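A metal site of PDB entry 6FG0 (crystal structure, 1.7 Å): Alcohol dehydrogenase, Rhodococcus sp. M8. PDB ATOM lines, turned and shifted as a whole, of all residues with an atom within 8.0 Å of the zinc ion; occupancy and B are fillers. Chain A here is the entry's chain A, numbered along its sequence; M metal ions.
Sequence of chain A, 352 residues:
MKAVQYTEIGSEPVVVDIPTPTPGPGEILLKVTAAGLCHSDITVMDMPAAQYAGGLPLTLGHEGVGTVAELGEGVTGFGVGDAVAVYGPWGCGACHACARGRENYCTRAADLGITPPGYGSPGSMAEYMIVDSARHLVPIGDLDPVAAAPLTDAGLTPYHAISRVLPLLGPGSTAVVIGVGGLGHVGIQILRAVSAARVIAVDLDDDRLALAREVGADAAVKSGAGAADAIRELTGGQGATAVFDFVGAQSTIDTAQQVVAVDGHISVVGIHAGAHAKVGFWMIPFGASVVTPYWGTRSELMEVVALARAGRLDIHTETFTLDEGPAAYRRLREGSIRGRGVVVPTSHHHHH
Gly 93 touches the zinc ion (N to ZN, 3.9 Å).
The nearest printed residue that does not touch the zinc ion is Thr 107 (4.3 Å).
SG of Cys 92 is bound to the zinc ion (2.3 Å).
The zinc ion is bound by SG of Cys 95, 2.3 Å away.
The side-chain sulfur (SG) of Cys 98 binds the zinc ion (2.4 Å).
SG of Cys 106 binds the zinc ion (2.4 Å).
The zinc ion has four donor atoms within binding distance.
The side-chain sulfur (SG) of Cys 98 lies close to the backbone NH (N) of Gly 93.
The side-chain sulfur (SG) of Cys 106 sits close to the backbone NH (N) of Ala 109, at 3.4 Å.
SG of Cys 106 lies close to N of Arg 108 (3.3 Å).
The side-chain sulfur of Cys 95 sits close to the side-chain hydroxyl of Thr 107 (3.8 Å).
The side-chain sulfur (SG) of Cys 92 sits close to the backbone NH (N) of Ala 94 (3.3 Å).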
ATOM      1  N   TRP A  90     -24.165  -7.326  24.460  1.00  0.00           N
ATOM      2  CA  TRP A  90     -23.611  -7.278  23.122  1.00  0.00           C
ATOM      3  C   TRP A  90     -24.256  -6.156  22.317  1.00  0.00           C
ATOM      4  O   TRP A  90     -25.487  -6.005  22.343  1.00  0.00           O
ATOM      5  CB  TRP A  90     -23.815  -8.624  22.412  1.00  0.00           C
ATOM      6  CG  TRP A  90     -23.054  -9.791  23.032  1.00  0.00           C
ATOM      7  CD1 TRP A  90     -22.114  -9.738  24.027  1.00  0.00           C
ATOM      8  CD2 TRP A  90     -23.169 -11.169  22.664  1.00  0.00           C
ATOM      9  NE1 TRP A  90     -21.653 -11.001  24.314  1.00  0.00           N
ATOM     10  CE2 TRP A  90     -22.293 -11.896  23.501  1.00  0.00           C
ATOM     11  CE3 TRP A  90     -23.961 -11.858  21.747  1.00  0.00           C
ATOM     12  CZ2 TRP A  90     -22.159 -13.279  23.422  1.00  0.00           C
ATOM     13  CZ3 TRP A  90     -23.831 -13.235  21.661  1.00  0.00           C
ATOM     14  CH2 TRP A  90     -22.949 -13.939  22.500  1.00  0.00           C
ATOM     15  N   GLY A  91     -23.424  -5.375  21.640  1.00  0.00           N
ATOM     16  CA  GLY A  91     -23.888  -4.342  20.707  1.00  0.00           C
ATOM     17  C   GLY A  91     -23.359  -4.538  19.322  1.00  0.00           C
ATOM     18  O   GLY A  91     -22.697  -5.553  19.032  1.00  0.00           O
ATOM     19  N   CYS A  92     -23.636  -3.567  18.443  1.00  0.00           N
ATOM     20  CA  CYS A  92     -23.285  -3.656  17.036  1.00  0.00           C
ATOM     21  C   CYS A  92     -21.780  -3.529  16.789  1.00  0.00           C
ATOM     22  O   CYS A  92     -21.282  -3.977  15.749  1.00  0.00           O
ATOM     23  CB  CYS A  92     -24.033  -2.593  16.204  1.00  0.00           C
ATOM     24  SG  CYS A  92     -23.452  -0.885  16.428  1.00  0.00           S
ATOM     25  N   GLY A  93     -21.064  -2.912  17.727  1.00  0.00           N
ATOM     26  CA  GLY A  93     -19.621  -2.717  17.632  1.00  0.00           C
ATOM     27  C   GLY A  93     -19.178  -1.515  16.807  1.00  0.00           C
ATOM     28  O   GLY A  93     -17.972  -1.198  16.783  1.00  0.00           O
ATOM     29  N   ALA A  94     -20.125  -0.836  16.128  1.00  0.00           N
ATOM     30  CA  ALA A  94     -19.806   0.158  15.085  1.00  0.00           C
ATOM     31  C   ALA A  94     -20.327   1.581  15.335  1.00  0.00           C
ATOM     32  O   ALA A  94     -19.761   2.537  14.786  1.00  0.00           O
ATOM     33  CB  ALA A  94     -20.342  -0.327  13.760  1.00  0.00           C
ATOM     34  N   CYS A  95     -21.381   1.727  16.134  1.00  0.00           N
ATOM     35  CA  CYS A  95     -21.975   3.028  16.402  1.00  0.00           C
ATOM     36  C   CYS A  95     -21.093   3.831  17.383  1.00  0.00           C
ATOM     37  O   CYS A  95     -20.108   3.313  17.927  1.00  0.00           O
ATOM     38  CB  CYS A  95     -23.379   2.863  17.021  1.00  0.00           C
ATOM     39  SG  CYS A  95     -23.429   2.187  18.670  1.00  0.00           S
ATOM     40  N   HIS A  96     -21.456   5.079  17.583  1.00  0.00           N
ATOM     41  CA  HIS A  96     -20.656   5.973  18.457  1.00  0.00           C
ATOM     42  C   HIS A  96     -20.502   5.470  19.891  1.00  0.00           C
ATOM     43  O   HIS A  96     -19.389   5.546  20.469  1.00  0.00           O
ATOM     44  CB  HIS A  96     -21.232   7.384  18.383  1.00  0.00           C
ATOM     45  CG  HIS A  96     -20.448   8.423  19.134  1.00  0.00           C
ATOM     46  ND1 HIS A  96     -20.717   8.737  20.438  1.00  0.00           N
ATOM     47  CD2 HIS A  96     -19.453   9.256  18.737  1.00  0.00           C
ATOM     48  CE1 HIS A  96     -19.901   9.714  20.839  1.00  0.00           C
ATOM     49  NE2 HIS A  96     -19.142  10.053  19.816  1.00  0.00           N
ATOM     50  N   ALA A  97     -21.593   4.966  20.501  1.00  0.00           N
ATOM     51  CA  ALA A  97     -21.515   4.318  21.800  1.00  0.00           C
ATOM     52  C   ALA A  97     -20.602   3.078  21.786  1.00  0.00           C
ATOM     53  O   ALA A  97     -19.715   2.960  22.654  1.00  0.00           O
ATOM     54  CB  ALA A  97     -22.904   3.939  22.321  1.00  0.00           C
ATOM     55  N   CYS A  98     -20.815   2.185  20.816  1.00  0.00           N
ATOM     56  CA  CYS A  98     -19.997   0.964  20.739  1.00  0.00           C
ATOM     57  C   CYS A  98     -18.505   1.281  20.487  1.00  0.00           C
ATOM     58  O   CYS A  98     -17.632   0.596  21.032  1.00  0.00           O
ATOM     59  CB  CYS A  98     -20.522  -0.020  19.665  1.00  0.00           C
ATOM     60  SG  CYS A  98     -22.049  -0.873  20.158  1.00  0.00           S
ATOM     61  N   ALA A  99     -18.235   2.316  19.704  1.00  0.00           N
ATOM     62  CA  ALA A  99     -16.844   2.712  19.427  1.00  0.00           C
ATOM     63  C   ALA A  99     -16.106   3.095  20.697  1.00  0.00           C
ATOM     64  O   ALA A  99     -14.896   2.943  20.775  1.00  0.00           O
ATOM     65  CB  ALA A  99     -16.805   3.844  18.406  1.00  0.00           C
ATOM     66  N   ARG A 102     -19.079   1.217  24.875  1.00  0.00           N
ATOM     67  CA  ARG A 102     -20.286   1.356  25.672  1.00  0.00           C
ATOM     68  C   ARG A 102     -21.403   0.589  24.979  1.00  0.00           C
ATOM     69  O   ARG A 102     -22.449   1.169  24.609  1.00  0.00           O
ATOM     70  CB  ARG A 102     -20.644   2.826  25.843  1.00  0.00           C
ATOM     71  CG  ARG A 102     -19.501   3.628  26.456  1.00  0.00           C
ATOM     72  CD  ARG A 102     -19.776   5.144  26.420  1.00  0.00           C
ATOM     73  NE  ARG A 102     -20.857   5.557  27.282  1.00  0.00           N
ATOM     74  CZ  ARG A 102     -20.792   5.672  28.611  1.00  0.00           C
ATOM     75  NH1 ARG A 102     -19.677   5.369  29.252  1.00  0.00           N
ATOM     76  NH2 ARG A 102     -21.846   6.060  29.318  1.00  0.00           N
ATOM     77  N   GLU A 103     -21.199  -0.707  24.787  1.00  0.00           N
ATOM     78  CA  GLU A 103     -22.156  -1.497  23.988  1.00  0.00           C
ATOM     79  C   GLU A 103     -23.476  -1.695  24.718  1.00  0.00           C
ATOM     80  O   GLU A 103     -24.511  -2.012  24.102  1.00  0.00           O
ATOM     81  CB  GLU A 103     -21.576  -2.837  23.559  1.00  0.00           C
ATOM     82  CG  GLU A 103     -20.277  -2.697  22.779  1.00  0.00           C
ATOM     83  CD  GLU A 103     -19.894  -3.931  21.981  1.00  0.00           C
ATOM     84  OE1 GLU A 103     -20.662  -4.913  21.881  1.00  0.00           O
ATOM     85  OE2 GLU A 103     -18.789  -3.902  21.380  1.00  0.00           O
ATOM     86  N   ASN A 104     -23.422  -1.516  26.035  1.00  0.00           N
ATOM     87  CA  ASN A 104     -24.633  -1.443  26.863  1.00  0.00           C
ATOM     88  C   ASN A 104     -25.601  -0.336  26.401  1.00  0.00           C
ATOM     89  O   ASN A 104     -26.823  -0.491  26.547  1.00  0.00           O
ATOM     90  CB  ASN A 104     -24.308  -1.314  28.355  1.00  0.00           C
ATOM     91  CG  ASN A 104     -23.394  -0.140  28.690  1.00  0.00           C
ATOM     92  OD1 ASN A 104     -22.520   0.237  27.917  1.00  0.00           O
ATOM     93  ND2 ASN A 104     -23.613   0.456  29.883  1.00  0.00           N
ATOM     94  N   TYR A 105     -25.067   0.729  25.818  1.00  0.00           N
ATOM     95  CA  TYR A 105     -25.879   1.841  25.288  1.00  0.00           C
ATOM     96  C   TYR A 105     -25.894   1.874  23.753  1.00  0.00           C
ATOM     97  O   TYR A 105     -26.121   2.923  23.145  1.00  0.00           O
ATOM     98  CB  TYR A 105     -25.373   3.164  25.906  1.00  0.00           C
ATOM     99  CG  TYR A 105     -25.521   3.207  27.413  1.00  0.00           C
ATOM    100  CD1 TYR A 105     -26.716   2.821  28.043  1.00  0.00           C
ATOM    101  CD2 TYR A 105     -24.483   3.678  28.219  1.00  0.00           C
ATOM    102  CE1 TYR A 105     -26.845   2.878  29.403  1.00  0.00           C
ATOM    103  CE2 TYR A 105     -24.602   3.717  29.600  1.00  0.00           C
ATOM    104  CZ  TYR A 105     -25.795   3.321  30.195  1.00  0.00           C
ATOM    105  OH  TYR A 105     -25.947   3.359  31.550  1.00  0.00           O
ATOM    106  N   CYS A 106     -25.710   0.707  23.130  1.00  0.00           N
ATOM    107  CA  CYS A 106     -25.732   0.602  21.679  1.00  0.00           C
ATOM    108  C   CYS A 106     -27.088   1.025  21.137  1.00  0.00           C
ATOM    109  O   CYS A 106     -28.120   0.572  21.638  1.00  0.00           O
ATOM    110  CB  CYS A 106     -25.487  -0.842  21.241  1.00  0.00           C
ATOM    111  SG  CYS A 106     -25.621  -1.080  19.464  1.00  0.00           S
ATOM    112  N   THR A 107     -27.085   1.869  20.121  1.00  0.00           N
ATOM    113  CA  THR A 107     -28.299   2.395  19.500  1.00  0.00           C
ATOM    114  C   THR A 107     -28.838   1.542  18.346  1.00  0.00           C
ATOM    115  O   THR A 107     -29.899   1.851  17.807  1.00  0.00           O
ATOM    116  CB  THR A 107     -28.029   3.824  18.977  1.00  0.00           C
ATOM    117  OG1 THR A 107     -26.776   3.840  18.283  1.00  0.00           O
ATOM    118  CG2 THR A 107     -27.907   4.792  20.145  1.00  0.00           C
ATOM    119  N   ARG A 108     -28.129   0.477  17.967  1.00  0.00           N
ATOM    120  CA  ARG A 108     -28.479  -0.331  16.803  1.00  0.00           C
ATOM    121  C   ARG A 108     -28.816  -1.801  17.119  1.00  0.00           C
ATOM    122  O   ARG A 108     -29.282  -2.522  16.228  1.00  0.00           O
ATOM    123  CB  ARG A 108     -27.330  -0.284  15.786  1.00  0.00           C
ATOM    124  CG  ARG A 108     -27.021   1.098  15.195  1.00  0.00           C
ATOM    125  CD  ARG A 108     -25.902   0.953  14.147  1.00  0.00           C
ATOM    126  NE  ARG A 108     -25.223   2.219  13.836  1.00  0.00           N
ATOM    127  CZ  ARG A 108     -24.067   2.349  13.155  1.00  0.00           C
ATOM    128  NH1 ARG A 108     -23.551   3.551  12.936  1.00  0.00           N
ATOM    129  NH2 ARG A 108     -23.409   1.283  12.704  1.00  0.00           N
ATOM    130  N   ALA A 109     -28.582  -2.242  18.361  1.00  0.00           N
ATOM    131  CA  ALA A 109     -28.703  -3.650  18.722  1.00  0.00           C
ATOM    132  C   ALA A 109     -30.109  -4.225  18.455  1.00  0.00           C
ATOM    133  O   ALA A 109     -30.233  -5.278  17.833  1.00  0.00           O
ATOM    134  CB  ALA A 109     -28.323  -3.864  20.187  1.00  0.00           C
ATOM    135  N   LEU A 112     -30.722  -4.644  14.671  1.00  0.00           N
ATOM    136  CA  LEU A 112     -29.919  -5.726  14.098  1.00  0.00           C
ATOM    137  C   LEU A 112     -30.226  -7.116  14.711  1.00  0.00           C
ATOM    138  O   LEU A 112     -29.633  -8.096  14.291  1.00  0.00           O
ATOM    139  CB  LEU A 112     -28.422  -5.391  14.200  1.00  0.00           C
ATOM    140  CG  LEU A 112     -27.991  -4.130  13.441  1.00  0.00           C
ATOM    141  CD1 LEU A 112     -26.569  -3.728  13.821  1.00  0.00           C
ATOM    142  CD2 LEU A 112     -28.101  -4.321  11.935  1.00  0.00           C
ATOM    143  N   ILE A 114     -29.585  -8.095  17.839  1.00  0.00           N
ATOM    144  CA  ILE A 114     -28.475  -8.519  18.673  1.00  0.00           C
ATOM    145  C   ILE A 114     -29.002  -8.603  20.092  1.00  0.00           C
ATOM    146  O   ILE A 114     -29.467  -7.600  20.633  1.00  0.00           O
ATOM    147  CB  ILE A 114     -27.284  -7.529  18.610  1.00  0.00           C
ATOM    148  CG1 ILE A 114     -26.711  -7.499  17.181  1.00  0.00           C
ATOM    149  CG2 ILE A 114     -26.196  -7.961  19.583  1.00  0.00           C
ATOM    150  CD1 ILE A 114     -25.737  -6.350  16.950  1.00  0.00           C
ATOM    151  N   ARG A 135     -14.060  -9.483  20.815  1.00  0.00           N
ATOM    152  CA  ARG A 135     -14.188  -8.268  21.615  1.00  0.00           C
ATOM    153  C   ARG A 135     -15.133  -8.446  22.813  1.00  0.00           C
ATOM    154  O   ARG A 135     -15.144  -7.597  23.702  1.00  0.00           O
ATOM    155  CB  ARG A 135     -14.607  -7.083  20.741  1.00  0.00           C
ATOM    156  CG  ARG A 135     -16.109  -6.986  20.443  1.00  0.00           C
ATOM    157  CD  ARG A 135     -16.409  -5.746  19.599  1.00  0.00           C
ATOM    158  NE  ARG A 135     -17.851  -5.588  19.471  1.00  0.00           N
ATOM    159  CZ  ARG A 135     -18.621  -6.236  18.603  1.00  0.00           C
ATOM    160  NH1 ARG A 135     -18.104  -7.107  17.719  1.00  0.00           N
ATOM    161  NH2 ARG A 135     -19.924  -6.009  18.602  1.00  0.00           N
HETATM  162 ZN    ZN M   1     -23.634  -0.129  18.589  1.00  0.00          ZN
